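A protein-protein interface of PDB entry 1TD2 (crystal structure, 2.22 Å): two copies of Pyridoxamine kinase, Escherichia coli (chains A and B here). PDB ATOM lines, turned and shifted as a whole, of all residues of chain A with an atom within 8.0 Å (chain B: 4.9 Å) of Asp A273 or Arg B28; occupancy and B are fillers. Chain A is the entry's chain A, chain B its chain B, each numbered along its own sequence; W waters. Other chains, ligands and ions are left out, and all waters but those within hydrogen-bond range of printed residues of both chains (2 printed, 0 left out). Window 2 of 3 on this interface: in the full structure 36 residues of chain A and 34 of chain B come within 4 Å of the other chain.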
ATOM      1  N   PHE A  24      -8.811   7.340 -13.573  1.00  0.00           N
ATOM      2  CA  PHE A  24      -9.336   8.052 -12.411  1.00  0.00           C
ATOM      3  C   PHE A  24     -10.673   8.746 -12.716  1.00  0.00           C
ATOM      4  O   PHE A  24     -11.651   8.546 -12.015  1.00  0.00           O
ATOM      5  CB  PHE A  24      -8.305   9.060 -11.830  1.00  0.00           C
ATOM      6  CG  PHE A  24      -8.797   9.739 -10.581  1.00  0.00           C
ATOM      7  CD1 PHE A  24      -9.264  11.051 -10.616  1.00  0.00           C
ATOM      8  CD2 PHE A  24      -8.896   9.021  -9.380  1.00  0.00           C
ATOM      9  CE1 PHE A  24      -9.826  11.636  -9.477  1.00  0.00           C
ATOM     10  CE2 PHE A  24      -9.451   9.592  -8.237  1.00  0.00           C
ATOM     11  CZ  PHE A  24      -9.915  10.892  -8.283  1.00  0.00           C
ATOM     12  N   ARG A  27     -13.604   6.151 -12.955  1.00  0.00           N
ATOM     13  CA  ARG A  27     -13.982   5.568 -11.706  1.00  0.00           C
ATOM     14  C   ARG A  27     -14.684   6.646 -10.876  1.00  0.00           C
ATOM     15  O   ARG A  27     -15.619   6.352 -10.142  1.00  0.00           O
ATOM     16  CB  ARG A  27     -12.736   5.034 -11.014  1.00  0.00           C
ATOM     17  CG  ARG A  27     -12.206   3.716 -11.614  1.00  0.00           C
ATOM     18  CD  ARG A  27     -10.935   3.264 -10.881  1.00  0.00           C
ATOM     19  NE  ARG A  27     -10.590   1.893 -11.221  1.00  0.00           N
ATOM     20  CZ  ARG A  27      -9.364   1.384 -11.156  1.00  0.00           C
ATOM     21  NH1 ARG A  27      -9.180   0.111 -11.480  1.00  0.00           N
ATOM     22  NH2 ARG A  27      -8.320   2.147 -10.794  1.00  0.00           N
ATOM     23  N   ARG A  28     -14.237   7.892 -11.026  1.00  0.00           N
ATOM     24  CA  ARG A  28     -14.812   9.040 -10.316  1.00  0.00           C
ATOM     25  C   ARG A  28     -16.273   9.172 -10.654  1.00  0.00           C
ATOM     26  O   ARG A  28     -17.064   9.636  -9.841  1.00  0.00           O
ATOM     27  CB  ARG A  28     -14.137  10.344 -10.738  1.00  0.00           C
ATOM     28  CG  ARG A  28     -13.590  11.235  -9.617  1.00  0.00           C
ATOM     29  CD  ARG A  28     -14.209  10.969  -8.270  1.00  0.00           C
ATOM     30  NE  ARG A  28     -14.482  12.205  -7.544  1.00  0.00           N
ATOM     31  CZ  ARG A  28     -15.689  12.542  -7.107  1.00  0.00           C
ATOM     32  NH1 ARG A  28     -16.726  11.731  -7.322  1.00  0.00           N
ATOM     33  NH2 ARG A  28     -15.865  13.684  -6.462  1.00  0.00           N
ATOM     34  N   LEU A  29     -16.611   8.804 -11.884  1.00  0.00           N
ATOM     35  CA  LEU A  29     -17.977   8.864 -12.336  1.00  0.00           C
ATOM     36  C   LEU A  29     -18.748   7.583 -12.000  1.00  0.00           C
ATOM     37  O   LEU A  29     -19.874   7.407 -12.450  1.00  0.00           O
ATOM     38  CB  LEU A  29     -18.050   9.142 -13.846  1.00  0.00           C
ATOM     39  CG  LEU A  29     -17.764  10.586 -14.299  1.00  0.00           C
ATOM     40  CD1 LEU A  29     -18.212  10.770 -15.753  1.00  0.00           C
ATOM     41  CD2 LEU A  29     -18.479  11.572 -13.387  1.00  0.00           C
ATOM     42  N   HIS A 246     -22.265  16.230 -20.648  1.00  0.00           N
ATOM     43  CA  HIS A 246     -21.482  15.982 -19.450  1.00  0.00           C
ATOM     44  C   HIS A 246     -19.984  15.841 -19.768  1.00  0.00           C
ATOM     45  O   HIS A 246     -19.142  16.467 -19.109  1.00  0.00           O
ATOM     46  CB  HIS A 246     -21.981  14.729 -18.708  1.00  0.00           C
ATOM     47  CG  HIS A 246     -21.369  14.549 -17.348  1.00  0.00           C
ATOM     48  ND1 HIS A 246     -21.744  13.538 -16.485  1.00  0.00           N
ATOM     49  CD2 HIS A 246     -20.412  15.259 -16.701  1.00  0.00           C
ATOM     50  CE1 HIS A 246     -21.044  13.638 -15.367  1.00  0.00           C
ATOM     51  NE2 HIS A 246     -20.228  14.674 -15.470  1.00  0.00           N
ATOM     52  N   GLU A 253     -13.442  21.409 -17.270  1.00  0.00           N
ATOM     53  CA  GLU A 253     -13.087  21.685 -15.860  1.00  0.00           C
ATOM     54  C   GLU A 253     -11.656  21.240 -15.597  1.00  0.00           C
ATOM     55  O   GLU A 253     -10.883  21.919 -14.911  1.00  0.00           O
ATOM     56  CB  GLU A 253     -14.019  20.923 -14.893  1.00  0.00           C
ATOM     57  CG  GLU A 253     -15.480  21.339 -14.943  1.00  0.00           C
ATOM     58  CD  GLU A 253     -15.720  22.749 -14.387  1.00  0.00           C
ATOM     59  OE1 GLU A 253     -16.884  23.192 -14.349  1.00  0.00           O
ATOM     60  OE2 GLU A 253     -14.749  23.409 -13.984  1.00  0.00           O
ATOM     61  N   GLN A 267      -4.574  17.832 -14.938  1.00  0.00           N
ATOM     62  CA  GLN A 267      -4.862  17.676 -13.513  1.00  0.00           C
ATOM     63  C   GLN A 267      -6.177  16.938 -13.244  1.00  0.00           C
ATOM     64  O   GLN A 267      -7.096  17.490 -12.640  1.00  0.00           O
ATOM     65  CB  GLN A 267      -4.871  19.070 -12.872  1.00  0.00           C
ATOM     66  CG  GLN A 267      -3.523  19.744 -12.966  1.00  0.00           C
ATOM     67  CD  GLN A 267      -2.427  18.917 -12.297  1.00  0.00           C
ATOM     68  OE1 GLN A 267      -1.422  18.551 -12.920  1.00  0.00           O
ATOM     69  NE2 GLN A 267      -2.625  18.615 -11.028  1.00  0.00           N
ATOM     70  N   VAL A 268      -6.244  15.687 -13.701  1.00  0.00           N
ATOM     71  CA  VAL A 268      -7.426  14.848 -13.555  1.00  0.00           C
ATOM     72  C   VAL A 268      -7.819  14.592 -12.107  1.00  0.00           C
ATOM     73  O   VAL A 268      -8.973  14.295 -11.817  1.00  0.00           O
ATOM     74  CB  VAL A 268      -7.227  13.488 -14.291  1.00  0.00           C
ATOM     75  CG1 VAL A 268      -7.275  13.708 -15.765  1.00  0.00           C
ATOM     76  CG2 VAL A 268      -5.865  12.865 -13.926  1.00  0.00           C
ATOM     77  N   VAL A 269      -6.855  14.731 -11.201  1.00  0.00           N
ATOM     78  CA  VAL A 269      -7.087  14.517  -9.783  1.00  0.00           C
ATOM     79  C   VAL A 269      -7.528  15.798  -9.062  1.00  0.00           C
ATOM     80  O   VAL A 269      -8.508  15.785  -8.326  1.00  0.00           O
ATOM     81  CB  VAL A 269      -5.817  13.933  -9.099  1.00  0.00           C
ATOM     82  CG1 VAL A 269      -6.006  13.886  -7.575  1.00  0.00           C
ATOM     83  CG2 VAL A 269      -5.536  12.514  -9.652  1.00  0.00           C
ATOM     84  N   ALA A 270      -6.813  16.897  -9.273  1.00  0.00           N
ATOM     85  CA  ALA A 270      -7.178  18.158  -8.642  1.00  0.00           C
ATOM     86  C   ALA A 270      -8.625  18.544  -8.985  1.00  0.00           C
ATOM     87  O   ALA A 270      -9.362  19.002  -8.125  1.00  0.00           O
ATOM     88  CB  ALA A 270      -6.211  19.276  -9.096  1.00  0.00           C
ATOM     89  N   ALA A 271      -9.047  18.326 -10.229  1.00  0.00           N
ATOM     90  CA  ALA A 271     -10.398  18.702 -10.627  1.00  0.00           C
ATOM     91  C   ALA A 271     -11.474  17.603 -10.477  1.00  0.00           C
ATOM     92  O   ALA A 271     -12.579  17.727 -10.994  1.00  0.00           O
ATOM     93  CB  ALA A 271     -10.350  19.206 -12.037  1.00  0.00           C
ATOM     94  N   GLN A 272     -11.166  16.540  -9.747  1.00  0.00           N
ATOM     95  CA  GLN A 272     -12.111  15.441  -9.576  1.00  0.00           C
ATOM     96  C   GLN A 272     -13.565  15.797  -9.209  1.00  0.00           C
ATOM     97  O   GLN A 272     -14.511  15.180  -9.726  1.00  0.00           O
ATOM     98  CB  GLN A 272     -11.560  14.438  -8.563  1.00  0.00           C
ATOM     99  CG  GLN A 272     -11.469  14.945  -7.138  1.00  0.00           C
ATOM    100  CD  GLN A 272     -10.953  13.860  -6.197  1.00  0.00           C
ATOM    101  OE1 GLN A 272     -11.684  12.929  -5.830  1.00  0.00           O
ATOM    102  NE2 GLN A 272      -9.682  13.964  -5.824  1.00  0.00           N
ATOM    103  N   ASP A 273     -13.776  16.782  -8.338  1.00  0.00           N
ATOM    104  CA  ASP A 273     -15.168  17.097  -8.007  1.00  0.00           C
ATOM    105  C   ASP A 273     -15.932  17.745  -9.151  1.00  0.00           C
ATOM    106  O   ASP A 273     -17.148  17.596  -9.258  1.00  0.00           O
ATOM    107  CB  ASP A 273     -15.284  18.004  -6.788  1.00  0.00           C
ATOM    108  CG  ASP A 273     -14.850  17.335  -5.498  1.00  0.00           C
ATOM    109  OD1 ASP A 273     -14.693  16.094  -5.455  1.00  0.00           O
ATOM    110  OD2 ASP A 273     -14.680  18.066  -4.510  1.00  0.00           O
ATOM    111  N   ARG A 274     -15.237  18.476 -10.011  1.00  0.00           N
ATOM    112  CA  ARG A 274     -15.944  19.127 -11.091  1.00  0.00           C
ATOM    113  C   ARG A 274     -16.076  18.200 -12.298  1.00  0.00           C
ATOM    114  O   ARG A 274     -16.683  18.542 -13.299  1.00  0.00           O
ATOM    115  CB  ARG A 274     -15.257  20.454 -11.403  1.00  0.00           C
ATOM    116  CG  ARG A 274     -15.393  21.422 -10.204  1.00  0.00           C
ATOM    117  CD  ARG A 274     -14.731  22.784 -10.402  1.00  0.00           C
ATOM    118  NE  ARG A 274     -13.294  22.636 -10.540  1.00  0.00           N
ATOM    119  CZ  ARG A 274     -12.500  22.240  -9.565  1.00  0.00           C
ATOM    120  NH1 ARG A 274     -13.013  21.965  -8.372  1.00  0.00           N
ATOM    121  NH2 ARG A 274     -11.208  22.095  -9.797  1.00  0.00           N
ATOM    122  N   ILE A 275     -15.509  17.006 -12.169  1.00  0.00           N
ATOM    123  CA  ILE A 275     -15.606  15.986 -13.197  1.00  0.00           C
ATOM    124  C   ILE A 275     -16.984  15.359 -12.948  1.00  0.00           C
ATOM    125  O   ILE A 275     -17.791  15.229 -13.863  1.00  0.00           O
ATOM    126  CB  ILE A 275     -14.508  14.903 -13.020  1.00  0.00           C
ATOM    127  CG1 ILE A 275     -13.137  15.490 -13.356  1.00  0.00           C
ATOM    128  CG2 ILE A 275     -14.825  13.694 -13.876  1.00  0.00           C
ATOM    129  CD1 ILE A 275     -11.974  14.499 -13.216  1.00  0.00           C
ATOM    130  N   ALA A 276     -17.266  14.997 -11.696  1.00  0.00           N
ATOM    131  CA  ALA A 276     -18.565  14.384 -11.374  1.00  0.00           C
ATOM    132  C   ALA A 276     -19.672  15.436 -11.410  1.00  0.00           C
ATOM    133  O   ALA A 276     -20.791  15.165 -11.864  1.00  0.00           O
ATOM    134  CB  ALA A 276     -18.518  13.681 -10.003  1.00  0.00           C
ATOM    135  N   LYS A 277     -19.349  16.647 -10.964  1.00  0.00           N
ATOM    136  CA  LYS A 277     -20.314  17.739 -10.971  1.00  0.00           C
ATOM    137  C   LYS A 277     -19.725  19.032 -11.563  1.00  0.00           C
ATOM    138  O   LYS A 277     -19.359  19.950 -10.830  1.00  0.00           O
ATOM    139  CB  LYS A 277     -20.824  18.013  -9.557  1.00  0.00           C
ATOM    140  CG  LYS A 277     -21.814  16.993  -9.010  1.00  0.00           C
ATOM    141  CD  LYS A 277     -22.599  17.583  -7.832  1.00  0.00           C
ATOM    142  CE  LYS A 277     -23.714  16.641  -7.366  1.00  0.00           C
ATOM    143  NZ  LYS A 277     -24.685  17.272  -6.406  1.00  0.00           N
ATOM    144  N   PRO A 278     -19.642  19.114 -12.900  1.00  0.00           N
ATOM    145  CA  PRO A 278     -19.107  20.280 -13.605  1.00  0.00           C
ATOM    146  C   PRO A 278     -19.901  21.534 -13.226  1.00  0.00           C
ATOM    147  O   PRO A 278     -21.109  21.464 -13.008  1.00  0.00           O
ATOM    148  CB  PRO A 278     -19.302  19.915 -15.077  1.00  0.00           C
ATOM    149  CG  PRO A 278     -19.365  18.414 -15.088  1.00  0.00           C
ATOM    150  CD  PRO A 278     -20.155  18.115 -13.861  1.00  0.00           C
ATOM    151  N   GLU A 279     -19.224  22.675 -13.171  1.00  0.00           N
ATOM    152  CA  GLU A 279     -19.869  23.936 -12.818  1.00  0.00           C
ATOM    153  C   GLU A 279     -20.107  24.822 -14.042  1.00  0.00           C
ATOM    154  O   GLU A 279     -20.624  25.925 -13.950  1.00  0.00           O
ATOM    155  CB  GLU A 279     -19.025  24.636 -11.760  1.00  0.00           C
ATOM    156  CG  GLU A 279     -18.972  23.803 -10.471  1.00  0.00           C
ATOM    157  CD  GLU A 279     -17.991  24.322  -9.431  1.00  0.00           C
ATOM    158  OE1 GLU A 279     -17.906  23.683  -8.356  1.00  0.00           O
ATOM    159  OE2 GLU A 279     -17.307  25.344  -9.679  1.00  0.00           O
ATOM    160  N   PHE B  24      -6.653   4.473  -6.511  1.00  0.00           N
ATOM    161  CA  PHE B  24      -7.869   5.250  -6.562  1.00  0.00           C
ATOM    162  C   PHE B  24      -8.229   5.892  -5.218  1.00  0.00           C
ATOM    163  O   PHE B  24      -8.373   7.136  -5.141  1.00  0.00           O
ATOM    164  CB  PHE B  24      -9.019   4.393  -7.116  1.00  0.00           C
ATOM    165  CG  PHE B  24     -10.329   5.128  -7.191  1.00  0.00           C
ATOM    166  CD1 PHE B  24     -11.325   4.902  -6.232  1.00  0.00           C
ATOM    167  CD2 PHE B  24     -10.525   6.131  -8.146  1.00  0.00           C
ATOM    168  CE1 PHE B  24     -12.478   5.667  -6.217  1.00  0.00           C
ATOM    169  CE2 PHE B  24     -11.675   6.897  -8.140  1.00  0.00           C
ATOM    170  CZ  PHE B  24     -12.655   6.671  -7.168  1.00  0.00           C
ATOM    171  N   PRO B  25      -8.347   5.087  -4.137  1.00  0.00           N
ATOM    172  CA  PRO B  25      -8.685   5.684  -2.835  1.00  0.00           C
ATOM    173  C   PRO B  25      -7.725   6.838  -2.469  1.00  0.00           C
ATOM    174  O   PRO B  25      -8.152   7.855  -1.932  1.00  0.00           O
ATOM    175  CB  PRO B  25      -8.574   4.507  -1.864  1.00  0.00           C
ATOM    176  CG  PRO B  25      -8.940   3.334  -2.717  1.00  0.00           C
ATOM    177  CD  PRO B  25      -8.203   3.619  -4.018  1.00  0.00           C
ATOM    178  N   MET B  26      -6.439   6.680  -2.770  1.00  0.00           N
ATOM    179  CA  MET B  26      -5.448   7.731  -2.457  1.00  0.00           C
ATOM    180  C   MET B  26      -5.681   9.000  -3.268  1.00  0.00           C
ATOM    181  O   MET B  26      -5.478  10.103  -2.787  1.00  0.00           O
ATOM    182  CB  MET B  26      -4.020   7.233  -2.726  1.00  0.00           C
ATOM    183  CG  MET B  26      -3.530   6.129  -1.760  1.00  0.00           C
ATOM    184  SD  MET B  26      -2.054   5.321  -2.380  1.00  0.00           S
ATOM    185  CE  MET B  26      -0.776   6.451  -1.679  1.00  0.00           C
ATOM    186  N   ARG B  27      -6.087   8.835  -4.516  1.00  0.00           N
ATOM    187  CA  ARG B  27      -6.351   9.982  -5.356  1.00  0.00           C
ATOM    188  C   ARG B  27      -7.666  10.648  -4.934  1.00  0.00           C
ATOM    189  O   ARG B  27      -7.789  11.877  -5.003  1.00  0.00           O
ATOM    190  CB  ARG B  27      -6.374   9.559  -6.839  1.00  0.00           C
ATOM    191  CG  ARG B  27      -4.996   9.201  -7.386  1.00  0.00           C
ATOM    192  CD  ARG B  27      -5.072   8.743  -8.852  1.00  0.00           C
ATOM    193  NE  ARG B  27      -3.749   8.737  -9.475  1.00  0.00           N
ATOM    194  CZ  ARG B  27      -3.431   8.071 -10.580  1.00  0.00           C
ATOM    195  NH1 ARG B  27      -2.179   8.143 -11.047  1.00  0.00           N
ATOM    196  NH2 ARG B  27      -4.353   7.319 -11.204  1.00  0.00           N
ATOM    197  N   ARG B  28      -8.630   9.847  -4.478  1.00  0.00           N
ATOM    198  CA  ARG B  28      -9.908  10.389  -4.023  1.00  0.00           C
ATOM    199  C   ARG B  28      -9.665  11.278  -2.813  1.00  0.00           C
ATOM    200  O   ARG B  28     -10.467  12.174  -2.524  1.00  0.00           O
ATOM    201  CB  ARG B  28     -10.925   9.280  -3.677  1.00  0.00           C
ATOM    202  CG  ARG B  28     -11.933   9.014  -4.801  1.00  0.00           C
ATOM    203  CD  ARG B  28     -13.360   9.578  -4.576  1.00  0.00           C
ATOM    204  NE  ARG B  28     -13.390  10.989  -4.222  1.00  0.00           N
ATOM    205  CZ  ARG B  28     -14.470  11.649  -3.814  1.00  0.00           C
ATOM    206  NH1 ARG B  28     -15.651  11.048  -3.712  1.00  0.00           N
ATOM    207  NH2 ARG B  28     -14.359  12.916  -3.467  1.00  0.00           N
ATOM    208  N   LEU B  29      -8.565  11.037  -2.106  1.00  0.00           N
ATOM    209  CA  LEU B  29      -8.241  11.884  -0.980  1.00  0.00           C
ATOM    210  C   LEU B  29      -7.422  13.103  -1.410  1.00  0.00           C
ATOM    211  O   LEU B  29      -6.903  13.843  -0.556  1.00  0.00           O
ATOM    212  CB  LEU B  29      -7.478  11.115   0.114  1.00  0.00           C
ATOM    213  CG  LEU B  29      -8.293  10.167   1.000  1.00  0.00           C
ATOM    214  CD1 LEU B  29      -7.601  10.058   2.333  1.00  0.00           C
ATOM    215  CD2 LEU B  29      -9.717  10.679   1.195  1.00  0.00           C
ATOM    216  N   GLY B  30      -7.245  13.290  -2.718  1.00  0.00           N
ATOM    217  CA  GLY B  30      -6.518  14.466  -3.174  1.00  0.00           C
ATOM    218  C   GLY B  30      -5.005  14.414  -3.282  1.00  0.00           C
ATOM    219  O   GLY B  30      -4.332  15.458  -3.326  1.00  0.00           O
ATOM    220  N   GLN B 272     -16.458   5.197  -2.866  1.00  0.00           N
ATOM    221  CA  GLN B 272     -15.618   6.392  -2.957  1.00  0.00           C
ATOM    222  C   GLN B 272     -16.000   7.646  -2.165  1.00  0.00           C
ATOM    223  O   GLN B 272     -15.113   8.332  -1.652  1.00  0.00           O
ATOM    224  CB  GLN B 272     -15.402   6.786  -4.423  1.00  0.00           C
ATOM    225  CG  GLN B 272     -16.632   7.304  -5.152  1.00  0.00           C
ATOM    226  CD  GLN B 272     -16.282   7.739  -6.559  1.00  0.00           C
ATOM    227  OE1 GLN B 272     -15.589   8.756  -6.762  1.00  0.00           O
ATOM    228  NE2 GLN B 272     -16.737   6.962  -7.549  1.00  0.00           N
ATOM    229  N   ASP B 273     -17.289   7.967  -2.070  1.00  0.00           N
ATOM    230  CA  ASP B 273     -17.689   9.164  -1.330  1.00  0.00           C
ATOM    231  C   ASP B 273     -17.491   9.028   0.159  1.00  0.00           C
ATOM    232  O   ASP B 273     -17.334  10.029   0.846  1.00  0.00           O
ATOM    233  CB  ASP B 273     -19.144   9.529  -1.592  1.00  0.00           C
ATOM    234  CG  ASP B 273     -19.379  10.012  -3.021  1.00  0.00           C
ATOM    235  OD1 ASP B 273     -18.392  10.171  -3.778  1.00  0.00           O
ATOM    236  OD2 ASP B 273     -20.551  10.229  -3.388  1.00  0.00           O
ATOM    237  N   ILE B 275     -14.967   7.279   1.429  1.00  0.00           N
ATOM    238  CA  ILE B 275     -13.537   7.114   1.663  1.00  0.00           C
ATOM    239  C   ILE B 275     -13.145   8.550   1.983  1.00  0.00           C
ATOM    240  O   ILE B 275     -12.401   8.811   2.915  1.00  0.00           O
ATOM    241  CB  ILE B 275     -12.776   6.647   0.375  1.00  0.00           C
ATOM    242  CG1 ILE B 275     -12.852   5.129   0.236  1.00  0.00           C
ATOM    243  CG2 ILE B 275     -11.334   7.088   0.408  1.00  0.00           C
ATOM    244  CD1 ILE B 275     -12.437   4.642  -1.129  1.00  0.00           C
ATOM    245  N   ALA B 276     -13.686   9.485   1.207  1.00  0.00           N
ATOM    246  CA  ALA B 276     -13.377  10.896   1.400  1.00  0.00           C
ATOM    247  C   ALA B 276     -14.069  11.432   2.637  1.00  0.00           C
ATOM    248  O   ALA B 276     -13.469  12.160   3.419  1.00  0.00           O
ATOM    249  CB  ALA B 276     -13.776  11.703   0.184  1.00  0.00           C
HETATM  250  O   HOH W   1      -7.014   1.848  -7.565  1.00  0.00           O
HETATM  251  O   HOH W   2      -6.089   7.805 -13.976  1.00  0.00           O
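The backbone carbonyl oxygen (O) of Arg A27 is in hydrogen-bond range of the side-chain amide nitrogen (NE2) of Gln B272 (2.9 Å). NH1 of Arg A28 sits close to OE1 of Gln B272 (3.2 Å). The side-chain amide nitrogen (NE2) of Gln A272 sits at hydrogen-bond distance from the backbone carbonyl oxygen (O) of Arg B27, at 2.9 Å. The side-chain amide oxygen (OE1) of Gln A272 lies within hydrogen-bond range of the guanidinium group (NE) of Arg B28, 3.0 Å away. The guanidinium group (NH2) of Arg B28 is in salt-bridge range of the side-chain carboxylate (OD1) of Asp A273. The guanidinium group of Arg B28 lies close to the guanidinium group of Arg A28 (3.4 Å).
NE of Arg A28 sits at hydrogen-bond distance from OE1 of Gln A272 (3.4 Å). The side-chain carboxylate of Asp A273 lies within salt-bridge range of the guanidinium group of Arg A28 (2.9 Å). The backbone carbonyl oxygen (O) of Val A269 lies close to the side-chain amide nitrogen (NE2) of Gln A272. The guanidinium group (NH1) of Arg B28 lies within hydrogen-bond range of the backbone carbonyl oxygen (O) of Gln B272 (3.5 Å). The guanidinium group of Arg B28 lies within salt-bridge range of the side-chain carboxylate of Asp B273 (2.9 Å).
CE2 of Phe A24 touches CE2 of Phe B24 (3.5 Å). Arg B27 touches Phe A24 (CB to CE2, 3.4 Å). Arg B28 touches Phe A24 (N to CE2, 3.9 Å). CE2 of Phe B24 touches CB of Arg A27, 3.6 Å away. Arg A28 touches Phe B24 (N to CE2, 3.99 Å). CG1 of Val A269 touches O of Arg B27 (3.7 Å).
Of the printed residues of chain B, Asp A273 touches Arg B28. Of chain A, only Phe A24, Arg A28, Gln A272 and Asp A273 come within 4 Å of Arg B28. Printed residues of chain B within 4 Å of Val A269: Arg B27. Printed residues of chain A within 4 Å of Gln B272: Arg A27 and Arg A28. Of the printed residues of chain B, Arg A27 touches Phe B24 and Gln B272. Of the printed residues of chain B, Phe A24 touches Phe B24 (3.5 Å), Arg B27 (3.4 Å) and Arg B28 (3.9 Å). Pro A278 touches none of the printed residues of chain B. Gly B30 touches none of the printed residues of chain A. The nearest residue of chain A that does not touch Arg B28 is Val A269 (5.7 Å). The nearest printed residue of chain B that does not touch Arg A27 is Arg B27 (6.5 Å).
Hydrophobic or aromatic side chains of chain A that line the printed part of chain B: Phe A24 and Val A269. Among the printed residues, 12 pairs touch across the chains.
Phe B24 touches its own counterpart, Phe A24. Arg A27 touches Gln B272, and with the chains exchanged Gln A272 touches Arg B27. Arg A28 touches Gln B272, and with the chains exchanged Gln A272 touches Arg B28. Asp A273 touches Arg B28, but with the chains exchanged Arg A28 does not touch Asp B273 (4.2 Å). Positions printed for both chains: 24, 27, 28, 29, 272, 273, 275 and 276. Of the 12 pairs that touch across the chains among the printed residues, 10 have their exchanged pair printed and touching as well.
Water W2 lies within hydrogen-bond range of N of Phe A24 (2.8 Å) and NH2 of Arg B27 (3.3 Å). Water W1 bridges N of Phe B24 and NH2 of Arg A27.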
